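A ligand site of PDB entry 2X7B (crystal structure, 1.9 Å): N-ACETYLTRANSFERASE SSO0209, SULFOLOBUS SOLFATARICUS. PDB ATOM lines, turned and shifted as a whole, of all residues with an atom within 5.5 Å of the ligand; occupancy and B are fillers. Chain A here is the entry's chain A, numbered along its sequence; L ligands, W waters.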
ATOM      1  N   THR A  33       0.436  18.225 -22.026  1.00  0.00           N
ATOM      2  CA  THR A  33       0.634  16.876 -21.496  1.00  0.00           C
ATOM      3  C   THR A  33       0.428  16.753 -19.992  1.00  0.00           C
ATOM      4  O   THR A  33       0.199  15.642 -19.484  1.00  0.00           O
ATOM      5  CB  THR A  33       2.050  16.348 -21.853  1.00  0.00           C
ATOM      6  OG1 THR A  33       3.027  17.283 -21.374  1.00  0.00           O
ATOM      7  CG2 THR A  33       2.218  16.158 -23.358  1.00  0.00           C
ATOM      8  N   LEU A  34       0.514  17.881 -19.285  1.00  0.00           N
ATOM      9  CA  LEU A  34       0.577  17.883 -17.818  1.00  0.00           C
ATOM     10  C   LEU A  34      -0.216  19.047 -17.225  1.00  0.00           C
ATOM     11  O   LEU A  34      -0.280  20.114 -17.826  1.00  0.00           O
ATOM     12  CB  LEU A  34       2.047  17.982 -17.345  1.00  0.00           C
ATOM     13  CG  LEU A  34       2.953  16.751 -17.573  1.00  0.00           C
ATOM     14  CD1 LEU A  34       4.429  17.156 -17.586  1.00  0.00           C
ATOM     15  CD2 LEU A  34       2.677  15.664 -16.538  1.00  0.00           C
ATOM     16  N   ILE A  93       8.982  15.520 -17.024  1.00  0.00           N
ATOM     17  CA  ILE A  93       9.333  14.808 -18.246  1.00  0.00           C
ATOM     18  C   ILE A  93       8.056  14.568 -19.067  1.00  0.00           C
ATOM     19  O   ILE A  93       7.027  14.160 -18.527  1.00  0.00           O
ATOM     20  CB  ILE A  93      10.113  13.478 -17.986  1.00  0.00           C
ATOM     21  CG1 ILE A  93      10.579  12.861 -19.312  1.00  0.00           C
ATOM     22  CG2 ILE A  93       9.285  12.464 -17.199  1.00  0.00           C
ATOM     23  CD1 ILE A  93      11.518  11.670 -19.155  1.00  0.00           C
ATOM     24  N   ALA A  94       8.122  14.854 -20.352  1.00  0.00           N
ATOM     25  CA  ALA A  94       6.969  14.679 -21.210  1.00  0.00           C
ATOM     26  C   ALA A  94       7.377  14.431 -22.655  1.00  0.00           C
ATOM     27  O   ALA A  94       8.413  14.905 -23.119  1.00  0.00           O
ATOM     28  CB  ALA A  94       6.055  15.895 -21.094  1.00  0.00           C
ATOM     29  N   VAL A  95       6.555  13.642 -23.344  1.00  0.00           N
ATOM     30  CA  VAL A  95       6.749  13.333 -24.773  1.00  0.00           C
ATOM     31  C   VAL A  95       5.398  13.575 -25.441  1.00  0.00           C
ATOM     32  O   VAL A  95       4.340  13.186 -24.890  1.00  0.00           O
ATOM     33  CB  VAL A  95       7.247  11.875 -24.993  1.00  0.00           C
ATOM     34  CG1 VAL A  95       7.443  11.552 -26.494  1.00  0.00           C
ATOM     35  CG2 VAL A  95       8.543  11.599 -24.219  1.00  0.00           C
ATOM     36  N   LEU A  96       5.428  14.243 -26.594  1.00  0.00           N
ATOM     37  CA  LEU A  96       4.209  14.464 -27.375  1.00  0.00           C
ATOM     38  C   LEU A  96       3.589  13.132 -27.757  1.00  0.00           C
ATOM     39  O   LEU A  96       4.294  12.196 -28.102  1.00  0.00           O
ATOM     40  CB  LEU A  96       4.497  15.270 -28.645  1.00  0.00           C
ATOM     41  CG  LEU A  96       4.769  16.755 -28.465  1.00  0.00           C
ATOM     42  CD1 LEU A  96       5.277  17.385 -29.778  1.00  0.00           C
ATOM     43  CD2 LEU A  96       3.566  17.521 -27.879  1.00  0.00           C
ATOM     44  N   TYR A  99       4.647  10.709 -30.573  1.00  0.00           N
ATOM     45  CA  TYR A  99       6.004  10.197 -30.509  1.00  0.00           C
ATOM     46  C   TYR A  99       6.253   9.269 -29.317  1.00  0.00           C
ATOM     47  O   TYR A  99       7.395   8.897 -29.048  1.00  0.00           O
ATOM     48  CB  TYR A  99       6.995  11.371 -30.528  1.00  0.00           C
ATOM     49  CG  TYR A  99       6.803  12.260 -31.742  1.00  0.00           C
ATOM     50  CD1 TYR A  99       7.320  11.892 -32.988  1.00  0.00           C
ATOM     51  CD2 TYR A  99       6.063  13.436 -31.648  1.00  0.00           C
ATOM     52  CE1 TYR A  99       7.116  12.709 -34.106  1.00  0.00           C
ATOM     53  CE2 TYR A  99       5.867  14.243 -32.748  1.00  0.00           C
ATOM     54  CZ  TYR A  99       6.399  13.881 -33.976  1.00  0.00           C
ATOM     55  OH  TYR A  99       6.183  14.704 -35.054  1.00  0.00           O
ATOM     56  N   ARG A 100       5.179   8.887 -28.638  1.00  0.00           N
ATOM     57  CA  ARG A 100       5.242   7.987 -27.485  1.00  0.00           C
ATOM     58  C   ARG A 100       5.485   6.525 -27.889  1.00  0.00           C
ATOM     59  O   ARG A 100       5.230   6.149 -29.031  1.00  0.00           O
ATOM     60  CB  ARG A 100       3.977   8.114 -26.634  1.00  0.00           C
ATOM     61  CG  ARG A 100       3.997   9.332 -25.728  1.00  0.00           C
ATOM     62  CD  ARG A 100       2.705   9.522 -24.945  1.00  0.00           C
ATOM     63  NE  ARG A 100       2.609  10.911 -24.516  1.00  0.00           N
ATOM     64  CZ  ARG A 100       1.535  11.473 -23.968  1.00  0.00           C
ATOM     65  NH1 ARG A 100       0.423  10.763 -23.728  1.00  0.00           N
ATOM     66  NH2 ARG A 100       1.576  12.757 -23.639  1.00  0.00           N
ATOM     67  N   ARG A 101       5.952   5.723 -26.929  1.00  0.00           N
ATOM     68  CA  ARG A 101       6.369   4.320 -27.130  1.00  0.00           C
ATOM     69  C   ARG A 101       7.449   4.121 -28.209  1.00  0.00           C
ATOM     70  O   ARG A 101       7.489   3.095 -28.875  1.00  0.00           O
ATOM     71  CB  ARG A 101       5.173   3.368 -27.421  1.00  0.00           C
ATOM     72  CG  ARG A 101       4.048   3.246 -26.389  1.00  0.00           C
ATOM     73  CD  ARG A 101       4.504   2.958 -24.956  1.00  0.00           C
ATOM     74  NE  ARG A 101       4.770   1.561 -24.592  1.00  0.00           N
ATOM     75  CZ  ARG A 101       3.871   0.652 -24.200  1.00  0.00           C
ATOM     76  NH1 ARG A 101       2.576   0.933 -24.191  1.00  0.00           N
ATOM     77  NH2 ARG A 101       4.268  -0.556 -23.843  1.00  0.00           N
ATOM     78  N   LYS A 102       8.313   5.113 -28.392  1.00  0.00           N
ATOM     79  CA  LYS A 102       9.459   4.977 -29.302  1.00  0.00           C
ATOM     80  C   LYS A 102      10.781   4.881 -28.528  1.00  0.00           C
ATOM     81  O   LYS A 102      11.859   4.792 -29.121  1.00  0.00           O
ATOM     82  CB  LYS A 102       9.522   6.136 -30.308  1.00  0.00           C
ATOM     83  CG  LYS A 102       8.426   6.127 -31.386  1.00  0.00           C
ATOM     84  CD  LYS A 102       8.507   7.347 -32.357  1.00  0.00           C
ATOM     85  CE  LYS A 102       9.945   7.703 -32.838  1.00  0.00           C
ATOM     86  NZ  LYS A 102      10.680   6.636 -33.641  1.00  0.00           N
ATOM     87  N   GLY A 103      10.678   4.897 -27.196  1.00  0.00           N
ATOM     88  CA  GLY A 103      11.857   4.895 -26.330  1.00  0.00           C
ATOM     89  C   GLY A 103      12.430   6.275 -26.042  1.00  0.00           C
ATOM     90  O   GLY A 103      13.571   6.389 -25.584  1.00  0.00           O
ATOM     91  N   ILE A 104      11.648   7.320 -26.303  1.00  0.00           N
ATOM     92  CA  ILE A 104      12.149   8.683 -26.163  1.00  0.00           C
ATOM     93  C   ILE A 104      12.359   9.019 -24.679  1.00  0.00           C
ATOM     94  O   ILE A 104      13.425   9.453 -24.278  1.00  0.00           O
ATOM     95  CB  ILE A 104      11.234   9.729 -26.816  1.00  0.00           C
ATOM     96  CG1 ILE A 104      11.228   9.580 -28.336  1.00  0.00           C
ATOM     97  CG2 ILE A 104      11.701  11.150 -26.485  1.00  0.00           C
ATOM     98  CD1 ILE A 104      10.303  10.568 -29.059  1.00  0.00           C
ATOM     99  N   ALA A 105      11.323   8.808 -23.854  1.00  0.00           N
ATOM    100  CA  ALA A 105      11.446   9.120 -22.424  1.00  0.00           C
ATOM    101  C   ALA A 105      12.566   8.324 -21.747  1.00  0.00           C
ATOM    102  O   ALA A 105      13.310   8.880 -20.940  1.00  0.00           O
ATOM    103  CB  ALA A 105      10.130   8.916 -21.701  1.00  0.00           C
ATOM    104  N   THR A 106      12.707   7.047 -22.125  1.00  0.00           N
ATOM    105  CA  THR A 106      13.781   6.197 -21.620  1.00  0.00           C
ATOM    106  C   THR A 106      15.117   6.813 -21.943  1.00  0.00           C
ATOM    107  O   THR A 106      15.966   6.928 -21.052  1.00  0.00           O
ATOM    108  CB  THR A 106      13.744   4.781 -22.236  1.00  0.00           C
ATOM    109  OG1 THR A 106      12.553   4.111 -21.824  1.00  0.00           O
ATOM    110  CG2 THR A 106      14.972   3.963 -21.777  1.00  0.00           C
ATOM    111  N   THR A 107      15.297   7.211 -23.193  1.00  0.00           N
ATOM    112  CA  THR A 107      16.535   7.834 -23.659  1.00  0.00           C
ATOM    113  C   THR A 107      16.792   9.156 -22.925  1.00  0.00           C
ATOM    114  O   THR A 107      17.929   9.438 -22.542  1.00  0.00           O
ATOM    115  CB  THR A 107      16.510   8.074 -25.191  1.00  0.00           C
ATOM    116  OG1 THR A 107      16.207   6.830 -25.860  1.00  0.00           O
ATOM    117  CG2 THR A 107      17.836   8.576 -25.688  1.00  0.00           C
ATOM    118  N   GLU A 128       8.401  12.329  -8.232  1.00  0.00           N
ATOM    119  CA  GLU A 128       7.045  12.082  -7.748  1.00  0.00           C
ATOM    120  C   GLU A 128       6.168  11.836  -8.966  1.00  0.00           C
ATOM    121  O   GLU A 128       6.362  12.449 -10.016  1.00  0.00           O
ATOM    122  CB  GLU A 128       6.472  13.285  -6.987  1.00  0.00           C
ATOM    123  CG  GLU A 128       7.345  13.844  -5.887  1.00  0.00           C
ATOM    124  CD  GLU A 128       8.506  14.693  -6.444  1.00  0.00           C
ATOM    125  OE1 GLU A 128       8.315  15.440  -7.437  1.00  0.00           O
ATOM    126  OE2 GLU A 128       9.616  14.586  -5.891  1.00  0.00           O
ATOM    127  N   VAL A 129       5.180  10.951  -8.805  1.00  0.00           N
ATOM    128  CA  VAL A 129       4.307  10.588  -9.909  1.00  0.00           C
ATOM    129  C   VAL A 129       2.910  10.314  -9.374  1.00  0.00           C
ATOM    130  O   VAL A 129       2.760   9.746  -8.287  1.00  0.00           O
ATOM    131  CB  VAL A 129       4.887   9.376 -10.689  1.00  0.00           C
ATOM    132  CG1 VAL A 129       5.099   8.177  -9.794  1.00  0.00           C
ATOM    133  CG2 VAL A 129       4.028   8.989 -11.898  1.00  0.00           C
ATOM    134  N   ARG A 130       1.876  10.693 -10.141  1.00  0.00           N
ATOM    135  CA  ARG A 130       0.473  10.392  -9.753  1.00  0.00           C
ATOM    136  C   ARG A 130       0.302   8.903  -9.648  1.00  0.00           C
ATOM    137  O   ARG A 130       0.835   8.182 -10.492  1.00  0.00           O
ATOM    138  CB  ARG A 130      -0.529  10.948 -10.772  1.00  0.00           C
ATOM    139  CG  ARG A 130      -0.622  12.428 -10.802  1.00  0.00           C
ATOM    140  CD  ARG A 130      -1.531  12.975 -11.917  1.00  0.00           C
ATOM    141  NE  ARG A 130      -1.571  14.437 -11.816  1.00  0.00           N
ATOM    142  CZ  ARG A 130      -2.453  15.139 -11.115  1.00  0.00           C
ATOM    143  NH1 ARG A 130      -3.429  14.529 -10.457  1.00  0.00           N
ATOM    144  NH2 ARG A 130      -2.374  16.472 -11.072  1.00  0.00           N
ATOM    145  N   ASN A 133      -0.861   7.289 -12.782  1.00  0.00           N
ATOM    146  CA  ASN A 133      -0.063   7.421 -13.984  1.00  0.00           C
ATOM    147  C   ASN A 133       0.728   6.148 -14.295  1.00  0.00           C
ATOM    148  O   ASN A 133       1.944   6.098 -14.164  1.00  0.00           O
ATOM    149  CB  ASN A 133       0.891   8.617 -13.853  1.00  0.00           C
ATOM    150  CG  ASN A 133       1.497   9.014 -15.179  1.00  0.00           C
ATOM    151  OD1 ASN A 133       1.406   8.278 -16.170  1.00  0.00           O
ATOM    152  ND2 ASN A 133       2.184  10.161 -15.191  1.00  0.00           N
ATOM    153  N   TYR A 134       0.011   5.113 -14.717  1.00  0.00           N
ATOM    154  CA  TYR A 134       0.636   3.819 -14.950  1.00  0.00           C
ATOM    155  C   TYR A 134       1.729   3.810 -16.035  1.00  0.00           C
ATOM    156  O   TYR A 134       2.682   3.068 -15.865  1.00  0.00           O
ATOM    157  CB  TYR A 134      -0.404   2.714 -15.187  1.00  0.00           C
ATOM    158  CG  TYR A 134      -1.277   2.407 -14.000  1.00  0.00           C
ATOM    159  CD1 TYR A 134      -0.874   1.488 -13.023  1.00  0.00           C
ATOM    160  CD2 TYR A 134      -2.545   3.016 -13.854  1.00  0.00           C
ATOM    161  CE1 TYR A 134      -1.708   1.196 -11.908  1.00  0.00           C
ATOM    162  CE2 TYR A 134      -3.373   2.734 -12.769  1.00  0.00           C
ATOM    163  CZ  TYR A 134      -2.956   1.816 -11.802  1.00  0.00           C
ATOM    164  OH  TYR A 134      -3.775   1.536 -10.714  1.00  0.00           O
ATOM    165  N   PRO A 135       1.589   4.599 -17.130  1.00  0.00           N
ATOM    166  CA  PRO A 135       2.645   4.581 -18.150  1.00  0.00           C
ATOM    167  C   PRO A 135       3.987   5.034 -17.576  1.00  0.00           C
ATOM    168  O   PRO A 135       5.032   4.451 -17.891  1.00  0.00           O
ATOM    169  CB  PRO A 135       2.141   5.578 -19.206  1.00  0.00           C
ATOM    170  CG  PRO A 135       0.640   5.488 -19.086  1.00  0.00           C
ATOM    171  CD  PRO A 135       0.418   5.379 -17.611  1.00  0.00           C
ATOM    172  N   ALA A 136       3.952   6.056 -16.737  1.00  0.00           N
ATOM    173  CA  ALA A 136       5.174   6.659 -16.190  1.00  0.00           C
ATOM    174  C   ALA A 136       5.739   5.786 -15.071  1.00  0.00           C
ATOM    175  O   ALA A 136       6.951   5.574 -14.988  1.00  0.00           O
ATOM    176  CB  ALA A 136       4.890   8.088 -15.690  1.00  0.00           C
ATOM    177  N   ALA A 138       5.459   2.585 -14.871  1.00  0.00           N
ATOM    178  CA  ALA A 138       6.119   1.527 -15.639  1.00  0.00           C
ATOM    179  C   ALA A 138       7.485   1.973 -16.199  1.00  0.00           C
ATOM    180  O   ALA A 138       8.461   1.259 -16.056  1.00  0.00           O
ATOM    181  CB  ALA A 138       5.217   1.013 -16.747  1.00  0.00           C
ATOM    182  N   LEU A 139       7.547   3.142 -16.834  1.00  0.00           N
ATOM    183  CA  LEU A 139       8.819   3.699 -17.296  1.00  0.00           C
ATOM    184  C   LEU A 139       9.853   3.723 -16.164  1.00  0.00           C
ATOM    185  O   LEU A 139      10.942   3.156 -16.311  1.00  0.00           O
ATOM    186  CB  LEU A 139       8.639   5.084 -17.922  1.00  0.00           C
ATOM    187  CG  LEU A 139       9.808   6.085 -18.100  1.00  0.00           C
ATOM    188  CD1 LEU A 139      10.784   5.717 -19.204  1.00  0.00           C
ATOM    189  CD2 LEU A 139       9.291   7.524 -18.323  1.00  0.00           C
ATOM    190  N   TYR A 140       9.500   4.316 -15.031  1.00  0.00           N
ATOM    191  CA  TYR A 140      10.444   4.501 -13.926  1.00  0.00           C
ATOM    192  C   TYR A 140      10.903   3.167 -13.317  1.00  0.00           C
ATOM    193  O   TYR A 140      12.086   2.991 -13.008  1.00  0.00           O
ATOM    194  CB  TYR A 140       9.855   5.403 -12.840  1.00  0.00           C
ATOM    195  CG  TYR A 140       9.394   6.750 -13.339  1.00  0.00           C
ATOM    196  CD1 TYR A 140      10.076   7.407 -14.348  1.00  0.00           C
ATOM    197  CD2 TYR A 140       8.271   7.372 -12.777  1.00  0.00           C
ATOM    198  CE1 TYR A 140       9.656   8.646 -14.798  1.00  0.00           C
ATOM    199  CE2 TYR A 140       7.841   8.609 -13.230  1.00  0.00           C
ATOM    200  CZ  TYR A 140       8.541   9.233 -14.237  1.00  0.00           C
ATOM    201  OH  TYR A 140       8.135  10.472 -14.660  1.00  0.00           O
ATOM    202  N   LYS A 142      11.111   0.293 -14.837  1.00  0.00           N
ATOM    203  CA  LYS A 142      12.067  -0.225 -15.830  1.00  0.00           C
ATOM    204  C   LYS A 142      13.486   0.323 -15.603  1.00  0.00           C
ATOM    205  O   LYS A 142      14.495  -0.397 -15.800  1.00  0.00           O
ATOM    206  CB  LYS A 142      11.597   0.138 -17.233  1.00  0.00           C
ATOM    207  CG  LYS A 142      12.213  -0.675 -18.375  1.00  0.00           C
ATOM    208  CD  LYS A 142      11.205  -0.919 -19.506  1.00  0.00           C
ATOM    209  CE  LYS A 142       9.890  -1.496 -18.951  1.00  0.00           C
ATOM    210  NZ  LYS A 142       9.057  -2.226 -19.949  1.00  0.00           N
ATOM    211  N   TYR A 155      -1.059  16.067  -5.178  1.00  0.00           N
ATOM    212  CA  TYR A 155      -1.447  16.924  -6.314  1.00  0.00           C
ATOM    213  C   TYR A 155      -2.583  17.858  -5.946  1.00  0.00           C
ATOM    214  O   TYR A 155      -3.337  17.563  -5.037  1.00  0.00           O
ATOM    215  CB  TYR A 155      -1.741  16.086  -7.556  1.00  0.00           C
ATOM    216  CG  TYR A 155      -0.473  15.409  -8.028  1.00  0.00           C
ATOM    217  CD1 TYR A 155       0.467  16.113  -8.784  1.00  0.00           C
ATOM    218  CD2 TYR A 155      -0.178  14.101  -7.645  1.00  0.00           C
ATOM    219  CE1 TYR A 155       1.660  15.495  -9.183  1.00  0.00           C
ATOM    220  CE2 TYR A 155       1.002  13.489  -8.042  1.00  0.00           C
ATOM    221  CZ  TYR A 155       1.902  14.198  -8.810  1.00  0.00           C
ATOM    222  OH  TYR A 155       3.071  13.604  -9.182  1.00  0.00           O
HETATM  223  N1  LIG L   1       1.114   1.973 -21.282  1.00  0.00           N
HETATM  224  C1  LIG L   1       1.855   1.100 -20.519  1.00  0.00           C
HETATM  225  N2  LIG L   1       3.209   1.336 -20.346  1.00  0.00           N
HETATM  226  C2  LIG L   1       3.810   2.419 -20.907  1.00  0.00           C
HETATM  227  C3  LIG L   1       3.076   3.308 -21.669  1.00  0.00           C
HETATM  228  C4  LIG L   1       1.705   3.080 -21.864  1.00  0.00           C
HETATM  229  N3  LIG L   1       1.021   3.802 -22.746  1.00  0.00           N
HETATM  230  N4  LIG L   1       3.921   4.273 -22.101  1.00  0.00           N
HETATM  231  C5  LIG L   1       5.164   4.012 -21.636  1.00  0.00           C
HETATM  232  N5  LIG L   1       5.110   2.858 -20.889  1.00  0.00           N
HETATM  233  C6  LIG L   1       6.214   2.239 -20.144  1.00  0.00           C
HETATM  234  C7  LIG L   1       6.566   0.875 -20.713  1.00  0.00           C
HETATM  235  O1  LIG L   1       6.937   0.058 -19.625  1.00  0.00           O
HETATM  236  C8  LIG L   1       7.794   1.202 -21.554  1.00  0.00           C
HETATM  237  O2  LIG L   1       8.661   0.115 -21.716  1.00  0.00           O
HETATM  238  P1  LIG L   1       8.411  -0.946 -22.908  1.00  0.00           P
HETATM  239  O3  LIG L   1       7.577  -0.357 -24.021  1.00  0.00           O
HETATM  240  O4  LIG L   1       7.683  -2.093 -22.259  1.00  0.00           O
HETATM  241  O5  LIG L   1       9.776  -1.394 -23.373  1.00  0.00           O
HETATM  242  C9  LIG L   1       8.481   2.298 -20.776  1.00  0.00           C
HETATM  243  O6  LIG L   1       7.385   3.029 -20.279  1.00  0.00           O
HETATM  244  C10 LIG L   1       9.407   3.167 -21.647  1.00  0.00           C
HETATM  245  O7  LIG L   1       8.629   3.787 -22.642  1.00  0.00           O
HETATM  246  P2  LIG L   1       9.167   5.002 -23.538  1.00  0.00           P
HETATM  247  O8  LIG L   1       8.710   4.809 -24.968  1.00  0.00           O
HETATM  248  O9  LIG L   1      10.634   5.257 -23.325  1.00  0.00           O
HETATM  249  O10 LIG L   1       8.239   6.195 -22.938  1.00  0.00           O
HETATM  250  P3  LIG L   1       7.548   7.376 -23.741  1.00  0.00           P
HETATM  251  O11 LIG L   1       8.606   7.995 -24.621  1.00  0.00           O
HETATM  252  O12 LIG L   1       6.259   7.001 -24.450  1.00  0.00           O
HETATM  253  O13 LIG L   1       7.105   8.440 -22.616  1.00  0.00           O
HETATM  254  C11 LIG L   1       5.824   9.268 -20.749  1.00  0.00           C
HETATM  255  C12 LIG L   1       6.453   8.046 -21.430  1.00  0.00           C
HETATM  256  C13 LIG L   1       6.890  10.370 -20.600  1.00  0.00           C
HETATM  257  C14 LIG L   1       5.298   8.854 -19.388  1.00  0.00           C
HETATM  258  C15 LIG L   1       4.649   9.705 -21.627  1.00  0.00           C
HETATM  259  O14 LIG L   1       3.631   8.728 -21.777  1.00  0.00           O
HETATM  260  C16 LIG L   1       4.087  11.072 -21.369  1.00  0.00           C
HETATM  261  O15 LIG L   1       4.660  12.131 -22.077  1.00  0.00           O
HETATM  262  N6  LIG L   1       3.069  11.220 -20.511  1.00  0.00           N
HETATM  263  C17 LIG L   1       2.545  12.543 -20.169  1.00  0.00           C
HETATM  264  C18 LIG L   1       3.494  13.348 -19.263  1.00  0.00           C
HETATM  265  C19 LIG L   1       3.812  12.586 -17.990  1.00  0.00           C
HETATM  266  O16 LIG L   1       2.924  11.905 -17.437  1.00  0.00           O
HETATM  267  N7  LIG L   1       5.051  12.662 -17.511  1.00  0.00           N
HETATM  268  C20 LIG L   1       5.405  12.123 -16.203  1.00  0.00           C
HETATM  269  C21 LIG L   1       4.958  12.967 -15.005  1.00  0.00           C
HETATM  270  S1  LIG L   1       5.687  12.415 -13.437  1.00  0.00           S
HETATM  271  O   HOH W   1       3.974   6.466 -23.500  1.00  0.00           O
HETATM  272  O   HOH W   2      -0.146  13.601 -21.800  1.00  0.00           O
HETATM  273  O   HOH W   3       1.490   6.000 -24.456  1.00  0.00           O
HETATM  274  O   HOH W   4       4.049  -0.986 -19.116  1.00  0.00           O
HETATM  275  O   HOH W   5       2.278  12.194 -12.848  1.00  0.00           O
HETATM  276  O   HOH W   6       1.569   9.262 -19.093  1.00  0.00           O
HETATM  277  O   HOH W   7       8.796   7.399 -27.132  1.00  0.00           O
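NH2 of Arg 101 is in salt-bridge range of O3 of the ligand, 3.3 Å away. The backbone carbonyl oxygen (O) of Ile 93 is in hydrogen-bond range of a nitrogen (N7) of the ligand, 2.7 Å away. The backbone NH (N) of Thr 106 lies within hydrogen-bond range of an oxygen (O9) of the ligand, at 3.0 Å. An oxygen (O8) of the ligand lies within hydrogen-bond range of the backbone NH (N) of Gly 103, 3.0 Å away. ND2 of Asn 133 lies within hydrogen-bond range of O16 of the ligand (2.9 Å). An oxygen (O6) of the ligand lies close to the backbone NH (N) of Leu 139 (3.5 Å). An oxygen (O9) of the ligand lies within hydrogen-bond range of the side-chain hydroxyl (OG1) of Thr 106 (2.7 Å). OH of Tyr 140 lies close to S1 of the ligand, at 3.4 Å. The backbone NH (N) of Ala 105 sits at hydrogen-bond distance from an oxygen (O11) of the ligand (2.9 Å). S1 of the ligand sits close to O of Glu 128 (3.5 Å). NZ of Lys 142 lies within salt-bridge range of O4 of the ligand, at 2.7 Å. O8 of the ligand lies within hydrogen-bond range of N of Lys 102. The backbone NH of Arg 101 sits at hydrogen-bond distance from an oxygen (O12) of the ligand (2.8 Å). N of Val 95 sits at hydrogen-bond distance from O15 of the ligand (2.7 Å). An oxygen (O15) of the ligand sits at hydrogen-bond distance from the guanidinium group of Arg 100, 3.4 Å away.
The backbone carbonyl oxygen (O) of Gly 103 sits at hydrogen-bond distance from the side-chain hydroxyl (OG1) of Thr 107, 2.7 Å away. OD1 of Asn 133 is in hydrogen-bond range of N of Ala 136, 3.4 Å away. The backbone carbonyl oxygen of Val 95 is in hydrogen-bond range of the guanidinium group of Arg 100, 2.9 Å away.
The backbone carbonyl oxygen of Pro 135 lies close to a nitrogen (N5) of the ligand, 3.4 Å away. Thr 33 touches the ligand (O to C17, 3.9 Å). Leu 34 touches the ligand (CD2 to C19, 3.6 Å). Ala 94 touches the ligand (CA to O15, 3.5 Å). N of Ile 104 touches O11 of the ligand (3.5 Å). Ala 136 touches the ligand. Ala 138 touches the ligand (CB to O1, 3.5 Å). Hydrophobic or aromatic side chains within 4 Å of the ligand: Leu 34, Val 95, Ile 104, Ala 105, Pro 135, Ala 136, Ala 138 and Leu 139. 20 residues have an atom within 4 Å of the ligand: Thr 33, Leu 34, Ile 93, Ala 94, Val 95, Arg 100, Arg 101, Lys 102, Gly 103, Ile 104, Ala 105, Thr 106, Glu 128, Asn 133, Pro 135, Ala 136, Ala 138, Leu 139, Tyr 140 and Lys 142.
Water W6 lies within hydrogen-bond range of a nitrogen (N6) of the ligand (2.8 Å) and the side-chain amide oxygen (OD1) of Asn 133 (3.1 Å). Water W2 bridges the guanidinium group of Arg 100 (2.7 Å) and the backbone carbonyl oxygen of Thr 33 (3.1 Å). Water W5 lies within hydrogen-bond range of ND2 of Asn 133 (3.1 Å), N of Arg 130 (3.1 Å) and S1 of the ligand (3.5 Å).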
